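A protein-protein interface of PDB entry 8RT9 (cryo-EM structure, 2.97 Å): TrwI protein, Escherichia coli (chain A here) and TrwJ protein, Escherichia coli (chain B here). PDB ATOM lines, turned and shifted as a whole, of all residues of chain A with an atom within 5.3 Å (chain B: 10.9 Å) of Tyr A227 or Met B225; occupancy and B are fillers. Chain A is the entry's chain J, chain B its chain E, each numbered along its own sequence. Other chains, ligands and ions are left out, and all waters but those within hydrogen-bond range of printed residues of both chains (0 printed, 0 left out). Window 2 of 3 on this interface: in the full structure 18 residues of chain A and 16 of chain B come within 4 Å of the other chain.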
ATOM      1  N   GLN A 222      17.964  16.017  11.296  1.00  0.00           N
ATOM      2  CA  GLN A 222      18.667  17.170  10.752  1.00  0.00           C
ATOM      3  C   GLN A 222      17.717  18.085   9.991  1.00  0.00           C
ATOM      4  O   GLN A 222      17.814  19.316  10.092  1.00  0.00           O
ATOM      5  CB  GLN A 222      19.811  16.707   9.858  1.00  0.00           C
ATOM      6  CG  GLN A 222      20.642  17.829   9.301  1.00  0.00           C
ATOM      7  CD  GLN A 222      20.296  18.143   7.864  1.00  0.00           C
ATOM      8  OE1 GLN A 222      20.059  17.244   7.059  1.00  0.00           O
ATOM      9  NE2 GLN A 222      20.264  19.428   7.531  1.00  0.00           N
ATOM     10  N   ILE A 223      16.782  17.506   9.235  1.00  0.00           N
ATOM     11  CA  ILE A 223      15.789  18.322   8.537  1.00  0.00           C
ATOM     12  C   ILE A 223      14.954  19.112   9.536  1.00  0.00           C
ATOM     13  O   ILE A 223      14.731  20.320   9.378  1.00  0.00           O
ATOM     14  CB  ILE A 223      14.906  17.439   7.639  1.00  0.00           C
ATOM     15  CG1 ILE A 223      15.668  17.017   6.389  1.00  0.00           C
ATOM     16  CG2 ILE A 223      13.638  18.168   7.260  1.00  0.00           C
ATOM     17  CD1 ILE A 223      14.994  15.921   5.620  1.00  0.00           C
ATOM     18  N   PHE A 224      14.489  18.436  10.587  1.00  0.00           N
ATOM     19  CA  PHE A 224      13.685  19.100  11.605  1.00  0.00           C
ATOM     20  C   PHE A 224      14.476  20.188  12.309  1.00  0.00           C
ATOM     21  O   PHE A 224      13.945  21.266  12.595  1.00  0.00           O
ATOM     22  CB  PHE A 224      13.176  18.073  12.611  1.00  0.00           C
ATOM     23  CG  PHE A 224      12.306  18.651  13.679  1.00  0.00           C
ATOM     24  CD1 PHE A 224      10.968  18.873  13.450  1.00  0.00           C
ATOM     25  CD2 PHE A 224      12.823  18.957  14.918  1.00  0.00           C
ATOM     26  CE1 PHE A 224      10.167  19.398  14.429  1.00  0.00           C
ATOM     27  CE2 PHE A 224      12.025  19.485  15.898  1.00  0.00           C
ATOM     28  CZ  PHE A 224      10.696  19.705  15.654  1.00  0.00           C
ATOM     29  N   GLY A 225      15.747  19.922  12.601  1.00  0.00           N
ATOM     30  CA  GLY A 225      16.572  20.921  13.247  1.00  0.00           C
ATOM     31  C   GLY A 225      16.762  22.156  12.396  1.00  0.00           C
ATOM     32  O   GLY A 225      16.691  23.277  12.896  1.00  0.00           O
ATOM     33  N   SER A 226      17.006  21.973  11.098  1.00  0.00           N
ATOM     34  CA  SER A 226      17.145  23.127  10.214  1.00  0.00           C
ATOM     35  C   SER A 226      15.854  23.930  10.159  1.00  0.00           C
ATOM     36  O   SER A 226      15.862  25.166  10.274  1.00  0.00           O
ATOM     37  CB  SER A 226      17.553  22.667   8.819  1.00  0.00           C
ATOM     38  OG  SER A 226      18.774  21.952   8.861  1.00  0.00           O
ATOM     39  N   TYR A 227      14.723  23.237  10.014  1.00  0.00           N
ATOM     40  CA  TYR A 227      13.446  23.934   9.943  1.00  0.00           C
ATOM     41  C   TYR A 227      13.197  24.744  11.204  1.00  0.00           C
ATOM     42  O   TYR A 227      12.810  25.914  11.135  1.00  0.00           O
ATOM     43  CB  TYR A 227      12.312  22.939   9.711  1.00  0.00           C
ATOM     44  CG  TYR A 227      10.953  23.586   9.627  1.00  0.00           C
ATOM     45  CD1 TYR A 227      10.204  23.825  10.763  1.00  0.00           C
ATOM     46  CD2 TYR A 227      10.420  23.953   8.410  1.00  0.00           C
ATOM     47  CE1 TYR A 227       8.972  24.416  10.690  1.00  0.00           C
ATOM     48  CE2 TYR A 227       9.186  24.541   8.330  1.00  0.00           C
ATOM     49  CZ  TYR A 227       8.467  24.770   9.473  1.00  0.00           C
ATOM     50  OH  TYR A 227       7.230  25.361   9.400  1.00  0.00           O
ATOM     51  N   MET A 228      13.412  24.141  12.373  1.00  0.00           N
ATOM     52  CA  MET A 228      13.200  24.883  13.610  1.00  0.00           C
ATOM     53  C   MET A 228      14.213  26.001  13.773  1.00  0.00           C
ATOM     54  O   MET A 228      13.882  27.056  14.321  1.00  0.00           O
ATOM     55  CB  MET A 228      13.244  23.952  14.816  1.00  0.00           C
ATOM     56  CG  MET A 228      12.179  22.892  14.804  1.00  0.00           C
ATOM     57  SD  MET A 228      10.549  23.608  14.590  1.00  0.00           S
ATOM     58  CE  MET A 228      10.207  24.135  16.253  1.00  0.00           C
ATOM     59  N   ALA A 229      15.442  25.800  13.308  1.00  0.00           N
ATOM     60  CA  ALA A 229      16.445  26.845  13.405  1.00  0.00           C
ATOM     61  C   ALA A 229      16.106  28.042  12.541  1.00  0.00           C
ATOM     62  O   ALA A 229      16.621  29.134  12.793  1.00  0.00           O
ATOM     63  CB  ALA A 229      17.815  26.297  13.017  1.00  0.00           C
ATOM     64  N   ASP A 230      15.265  27.869  11.529  1.00  0.00           N
ATOM     65  CA  ASP A 230      14.830  29.013  10.738  1.00  0.00           C
ATOM     66  C   ASP A 230      13.535  29.641  11.244  1.00  0.00           C
ATOM     67  O   ASP A 230      13.063  30.611  10.646  1.00  0.00           O
ATOM     68  CB  ASP A 230      14.665  28.606   9.275  1.00  0.00           C
ATOM     69  CG  ASP A 230      14.730  29.788   8.333  1.00  0.00           C
ATOM     70  OD1 ASP A 230      15.595  30.664   8.541  1.00  0.00           O
ATOM     71  OD2 ASP A 230      13.916  29.845   7.388  1.00  0.00           O
ATOM     72  N   LEU A 231      12.955  29.130  12.326  1.00  0.00           N
ATOM     73  CA  LEU A 231      11.689  29.646  12.832  1.00  0.00           C
ATOM     74  C   LEU A 231      11.912  30.897  13.668  1.00  0.00           C
ATOM     75  O   LEU A 231      12.850  30.969  14.465  1.00  0.00           O
ATOM     76  CB  LEU A 231      10.983  28.580  13.666  1.00  0.00           C
ATOM     77  CG  LEU A 231       9.509  28.770  13.999  1.00  0.00           C
ATOM     78  CD1 LEU A 231       8.814  27.435  13.984  1.00  0.00           C
ATOM     79  CD2 LEU A 231       9.342  29.423  15.351  1.00  0.00           C
ATOM     80  N   GLN A 237       6.787  36.308   9.618  1.00  0.00           N
ATOM     81  CA  GLN A 237       6.510  34.887   9.513  1.00  0.00           C
ATOM     82  C   GLN A 237       5.147  34.585  10.110  1.00  0.00           C
ATOM     83  O   GLN A 237       4.833  35.031  11.215  1.00  0.00           O
ATOM     84  CB  GLN A 237       7.582  34.070  10.229  1.00  0.00           C
ATOM     85  CG  GLN A 237       8.676  33.569   9.323  1.00  0.00           C
ATOM     86  CD  GLN A 237       9.508  32.496   9.970  1.00  0.00           C
ATOM     87  OE1 GLN A 237       9.022  31.745  10.810  1.00  0.00           O
ATOM     88  NE2 GLN A 237      10.768  32.409   9.576  1.00  0.00           N
ATOM     89  N   ASN A 238       4.340  33.829   9.376  1.00  0.00           N
ATOM     90  CA  ASN A 238       3.034  33.436   9.878  1.00  0.00           C
ATOM     91  C   ASN A 238       3.210  32.390  10.962  1.00  0.00           C
ATOM     92  O   ASN A 238       3.791  31.328  10.720  1.00  0.00           O
ATOM     93  CB  ASN A 238       2.170  32.892   8.748  1.00  0.00           C
ATOM     94  CG  ASN A 238       0.698  33.003   9.045  1.00  0.00           C
ATOM     95  OD1 ASN A 238       0.305  33.484  10.103  1.00  0.00           O
ATOM     96  ND2 ASN A 238      -0.129  32.560   8.112  1.00  0.00           N
ATOM     97  N   TYR A 241       1.567  29.031  10.101  1.00  0.00           N
ATOM     98  CA  TYR A 241       2.330  28.270   9.117  1.00  0.00           C
ATOM     99  C   TYR A 241       3.528  27.592   9.763  1.00  0.00           C
ATOM    100  O   TYR A 241       3.799  26.413   9.512  1.00  0.00           O
ATOM    101  CB  TYR A 241       2.800  29.184   7.988  1.00  0.00           C
ATOM    102  CG  TYR A 241       1.728  29.650   7.044  1.00  0.00           C
ATOM    103  CD1 TYR A 241       0.427  29.213   7.165  1.00  0.00           C
ATOM    104  CD2 TYR A 241       2.025  30.536   6.026  1.00  0.00           C
ATOM    105  CE1 TYR A 241      -0.546  29.647   6.300  1.00  0.00           C
ATOM    106  CE2 TYR A 241       1.061  30.972   5.162  1.00  0.00           C
ATOM    107  CZ  TYR A 241      -0.220  30.527   5.302  1.00  0.00           C
ATOM    108  OH  TYR A 241      -1.187  30.963   4.434  1.00  0.00           O
ATOM    109  N   ALA A 242       4.254  28.322  10.606  1.00  0.00           N
ATOM    110  CA  ALA A 242       5.465  27.781  11.207  1.00  0.00           C
ATOM    111  C   ALA A 242       5.151  26.639  12.165  1.00  0.00           C
ATOM    112  O   ALA A 242       5.777  25.573  12.105  1.00  0.00           O
ATOM    113  CB  ALA A 242       6.226  28.893  11.923  1.00  0.00           C
ATOM    114  N   ILE A 243       4.185  26.840  13.061  1.00  0.00           N
ATOM    115  CA  ILE A 243       3.844  25.789  14.016  1.00  0.00           C
ATOM    116  C   ILE A 243       3.269  24.578  13.294  1.00  0.00           C
ATOM    117  O   ILE A 243       3.534  23.427  13.668  1.00  0.00           O
ATOM    118  CB  ILE A 243       2.878  26.326  15.084  1.00  0.00           C
ATOM    119  CG1 ILE A 243       3.466  27.561  15.759  1.00  0.00           C
ATOM    120  CG2 ILE A 243       2.583  25.260  16.118  1.00  0.00           C
ATOM    121  CD1 ILE A 243       4.461  27.250  16.832  1.00  0.00           C
ATOM    122  N   GLY A 244       2.479  24.811  12.247  1.00  0.00           N
ATOM    123  CA  GLY A 244       1.957  23.701  11.475  1.00  0.00           C
ATOM    124  C   GLY A 244       3.048  22.922  10.773  1.00  0.00           C
ATOM    125  O   GLY A 244       3.012  21.693  10.737  1.00  0.00           O
ATOM    126  N   GLY A 245       4.025  23.619  10.201  1.00  0.00           N
ATOM    127  CA  GLY A 245       5.150  22.923   9.611  1.00  0.00           C
ATOM    128  C   GLY A 245       5.908  22.104  10.632  1.00  0.00           C
ATOM    129  O   GLY A 245       6.325  20.978  10.355  1.00  0.00           O
ATOM    130  N   SER A 246       6.077  22.651  11.835  1.00  0.00           N
ATOM    131  CA  SER A 246       6.758  21.909  12.888  1.00  0.00           C
ATOM    132  C   SER A 246       6.014  20.624  13.221  1.00  0.00           C
ATOM    133  O   SER A 246       6.613  19.543  13.274  1.00  0.00           O
ATOM    134  CB  SER A 246       6.903  22.777  14.134  1.00  0.00           C
ATOM    135  OG  SER A 246       5.638  23.068  14.697  1.00  0.00           O
ATOM    136  N   LEU A 249       6.182  18.062  10.278  1.00  0.00           N
ATOM    137  CA  LEU A 249       7.477  17.395  10.200  1.00  0.00           C
ATOM    138  C   LEU A 249       7.637  16.386  11.323  1.00  0.00           C
ATOM    139  O   LEU A 249       8.085  15.254  11.095  1.00  0.00           O
ATOM    140  CB  LEU A 249       8.600  18.426  10.248  1.00  0.00           C
ATOM    141  CG  LEU A 249       8.900  19.169   8.951  1.00  0.00           C
ATOM    142  CD1 LEU A 249      10.031  20.139   9.166  1.00  0.00           C
ATOM    143  CD2 LEU A 249       9.241  18.195   7.852  1.00  0.00           C
ATOM    144  N   ILE B 217       2.653  40.437  15.393  1.00  0.00           N
ATOM    145  CA  ILE B 217       3.219  39.090  15.406  1.00  0.00           C
ATOM    146  C   ILE B 217       2.217  38.075  14.870  1.00  0.00           C
ATOM    147  O   ILE B 217       2.571  37.192  14.082  1.00  0.00           O
ATOM    148  CB  ILE B 217       3.694  38.720  16.820  1.00  0.00           C
ATOM    149  CG1 ILE B 217       4.949  39.501  17.180  1.00  0.00           C
ATOM    150  CG2 ILE B 217       3.972  37.247  16.912  1.00  0.00           C
ATOM    151  CD1 ILE B 217       5.427  39.247  18.579  1.00  0.00           C
ATOM    152  N   SER B 219      -0.509  38.548  12.972  1.00  0.00           N
ATOM    153  CA  SER B 219      -1.323  38.981  11.846  1.00  0.00           C
ATOM    154  C   SER B 219      -1.470  37.868  10.822  1.00  0.00           C
ATOM    155  O   SER B 219      -0.511  37.160  10.506  1.00  0.00           O
ATOM    156  CB  SER B 219      -0.705  40.209  11.189  1.00  0.00           C
ATOM    157  OG  SER B 219      -1.524  40.690  10.141  1.00  0.00           O
ATOM    158  N   GLY B 221      -2.025  38.404   7.746  1.00  0.00           N
ATOM    159  CA  GLY B 221      -1.440  38.835   6.497  1.00  0.00           C
ATOM    160  C   GLY B 221      -0.009  38.411   6.297  1.00  0.00           C
ATOM    161  O   GLY B 221       0.535  38.605   5.207  1.00  0.00           O
ATOM    162  N   ASN B 222       0.615  37.842   7.321  1.00  0.00           N
ATOM    163  CA  ASN B 222       1.969  37.339   7.182  1.00  0.00           C
ATOM    164  C   ASN B 222       1.988  36.155   6.230  1.00  0.00           C
ATOM    165  O   ASN B 222       1.048  35.358   6.187  1.00  0.00           O
ATOM    166  CB  ASN B 222       2.521  36.932   8.542  1.00  0.00           C
ATOM    167  CG  ASN B 222       2.565  38.081   9.509  1.00  0.00           C
ATOM    168  OD1 ASN B 222       2.590  39.239   9.108  1.00  0.00           O
ATOM    169  ND2 ASN B 222       2.574  37.771  10.794  1.00  0.00           N
ATOM    170  N   GLN B 223       3.066  36.040   5.459  1.00  0.00           N
ATOM    171  CA  GLN B 223       3.158  35.027   4.424  1.00  0.00           C
ATOM    172  C   GLN B 223       4.389  34.145   4.544  1.00  0.00           C
ATOM    173  O   GLN B 223       4.557  33.232   3.731  1.00  0.00           O
ATOM    174  CB  GLN B 223       3.142  35.687   3.042  1.00  0.00           C
ATOM    175  CG  GLN B 223       1.789  36.222   2.633  1.00  0.00           C
ATOM    176  CD  GLN B 223       0.768  35.124   2.433  1.00  0.00           C
ATOM    177  OE1 GLN B 223       0.083  34.715   3.370  1.00  0.00           O
ATOM    178  NE2 GLN B 223       0.658  34.639   1.202  1.00  0.00           N
ATOM    179  N   GLY B 224       5.245  34.379   5.521  1.00  0.00           N
ATOM    180  CA  GLY B 224       6.489  33.651   5.604  1.00  0.00           C
ATOM    181  C   GLY B 224       6.397  32.395   6.441  1.00  0.00           C
ATOM    182  O   GLY B 224       5.476  32.207   7.228  1.00  0.00           O
ATOM    183  N   MET B 225       7.381  31.526   6.252  1.00  0.00           N
ATOM    184  CA  MET B 225       7.547  30.331   7.063  1.00  0.00           C
ATOM    185  C   MET B 225       8.952  29.798   6.833  1.00  0.00           C
ATOM    186  O   MET B 225       9.601  30.173   5.853  1.00  0.00           O
ATOM    187  CB  MET B 225       6.500  29.266   6.715  1.00  0.00           C
ATOM    188  CG  MET B 225       6.550  28.776   5.294  1.00  0.00           C
ATOM    189  SD  MET B 225       5.357  27.462   5.056  1.00  0.00           S
ATOM    190  CE  MET B 225       6.091  26.174   6.047  1.00  0.00           C
ATOM    191  N   PRO B 226       9.456  28.944   7.720  1.00  0.00           N
ATOM    192  CA  PRO B 226      10.792  28.384   7.514  1.00  0.00           C
ATOM    193  C   PRO B 226      10.853  27.540   6.253  1.00  0.00           C
ATOM    194  O   PRO B 226       9.864  26.946   5.821  1.00  0.00           O
ATOM    195  CB  PRO B 226      11.015  27.532   8.765  1.00  0.00           C
ATOM    196  CG  PRO B 226      10.118  28.120   9.775  1.00  0.00           C
ATOM    197  CD  PRO B 226       8.904  28.542   9.021  1.00  0.00           C
ATOM    198  N   THR B 227      12.038  27.495   5.657  1.00  0.00           N
ATOM    199  CA  THR B 227      12.271  26.759   4.425  1.00  0.00           C
ATOM    200  C   THR B 227      13.116  25.530   4.712  1.00  0.00           C
ATOM    201  O   THR B 227      14.078  25.595   5.483  1.00  0.00           O
ATOM    202  CB  THR B 227      12.966  27.637   3.387  1.00  0.00           C
ATOM    203  OG1 THR B 227      14.206  28.111   3.920  1.00  0.00           O
ATOM    204  CG2 THR B 227      12.092  28.825   3.029  1.00  0.00           C
ATOM    205  N   ILE B 228      12.752  24.410   4.097  1.00  0.00           N
ATOM    206  CA  ILE B 228      13.530  23.185   4.207  1.00  0.00           C
ATOM    207  C   ILE B 228      14.622  23.210   3.149  1.00  0.00           C
ATOM    208  O   ILE B 228      14.339  23.325   1.952  1.00  0.00           O
ATOM    209  CB  ILE B 228      12.640  21.946   4.048  1.00  0.00           C
ATOM    210  CG1 ILE B 228      11.538  21.942   5.099  1.00  0.00           C
ATOM    211  CG2 ILE B 228      13.466  20.687   4.154  1.00  0.00           C
ATOM    212  CD1 ILE B 228      10.657  20.728   5.036  1.00  0.00           C
ATOM    213  N   GLN B 229      15.870  23.102   3.587  1.00  0.00           N
ATOM    214  CA  GLN B 229      17.000  23.129   2.671  1.00  0.00           C
ATOM    215  C   GLN B 229      18.113  22.202   3.146  1.00  0.00           C
ATOM    216  O   GLN B 229      17.850  21.142   3.712  1.00  0.00           O
ATOM    217  CB  GLN B 229      17.531  24.556   2.519  1.00  0.00           C
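The side-chain amide nitrogen (NE2) of Gln A237 lies within hydrogen-bond range of the backbone carbonyl oxygen (O) of Asp A230. The side-chain amide nitrogen (ND2) of Asn B222 lies within hydrogen-bond range of the backbone carbonyl oxygen (O) of Ile B217, at 3.3 Å. N of Gly B221 lies close to OG of Ser B219 (3.3 Å). O of Ser B219 sits at hydrogen-bond distance from ND2 of Asn B222, at 3.2 Å. O of Ala A242 is in hydrogen-bond range of OH of Tyr A227 (3.1 Å).
Hydrophobic or aromatic side chains of chain A within 4 Å of the printed part of chain B: Tyr A227, Tyr A241 and Ala A242. Printed residues of chain B that touch a printed residue of chain A: Ser B219, Asn B222, Gly B224, Met B225, Pro B226 and Thr B227. Hydrophobic or aromatic side chains of chain B that line the printed part of chain A: Met B225 and Pro B226. Among the printed residues, 14 pairs touch across the chains. Among the printed residues, no Asp or Glu carboxylate lies within 4 Å of a Lys or Arg side-chain nitrogen of the other chain.
Met B225 touches just these residues of chain A: Tyr A227, Gln A237 and Tyr A241. No residue of chain B comes within 4 Å of Gly A225. No residue of chain B comes within 4 Å of Ser A226. No residue of chain B comes within 4 Å of Met A228. No residue of chain B comes within 4 Å of Ala A229. Of chain B, only Pro B226 and Thr B227 come within 4 Å of Asp A230. Leu A231 touches just one residue of chain B: Pro B226 (3.8 Å). Of chain B, only Asn B222 (3.6 Å), Gly B224 (3.7 Å), Met B225 (3.9 Å) and Pro B226 (3.7 Å) come within 4 Å of Gln A237. Of chain B, only Pro B226 (3.96 Å) comes within 4 Å of Ala A242. No residue of chain B comes within 4 Å of Gly A244. No residue of chain B comes within 4 Å of Gly A245. No residue of chain B comes within 4 Å of Ser A246. Of the printed residues of chain A, Thr B227 touches Asp A230. Printed residues of chain A within 4 Å of Pro B226: Tyr A227, Asp A230, Leu A231, Gln A237 and Ala A242. Ile A223 touches none of the printed residues of chain B. The nearest residue of chain B that does not touch Tyr A227 is Ile B228 (4.03 Å).
The backbone NH (N) of Thr B227 sits at hydrogen-bond distance from the side-chain carboxylate (OD2) of Asp A230 (3.5 Å). The backbone carbonyl oxygen (O) of Gly B224 sits at hydrogen-bond distance from the backbone NH (N) of Asn A238 (2.9 Å).
Met B225 touches Tyr A227 (CE to OH, 3.6 Å). Tyr A227 touches Pro B226 (O to CB, 3.4 Å). Asp A230 touches Pro B226. O of Gln A237 touches ND2 of Asn B222, 3.6 Å away. CA of Gln A237 touches O of Gly B224, 3.7 Å away. Gln A237 touches Met B225 (CG to N, 3.9 Å). Pro B226 touches Gln A237. Asn A238 touches Ser B219 (OD1 to O, 3.8 Å). CB of Met B225 touches CB of Tyr A241, at 3.9 Å. Pro B226 touches Ala A242 (CD to CB, 3.96 Å).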
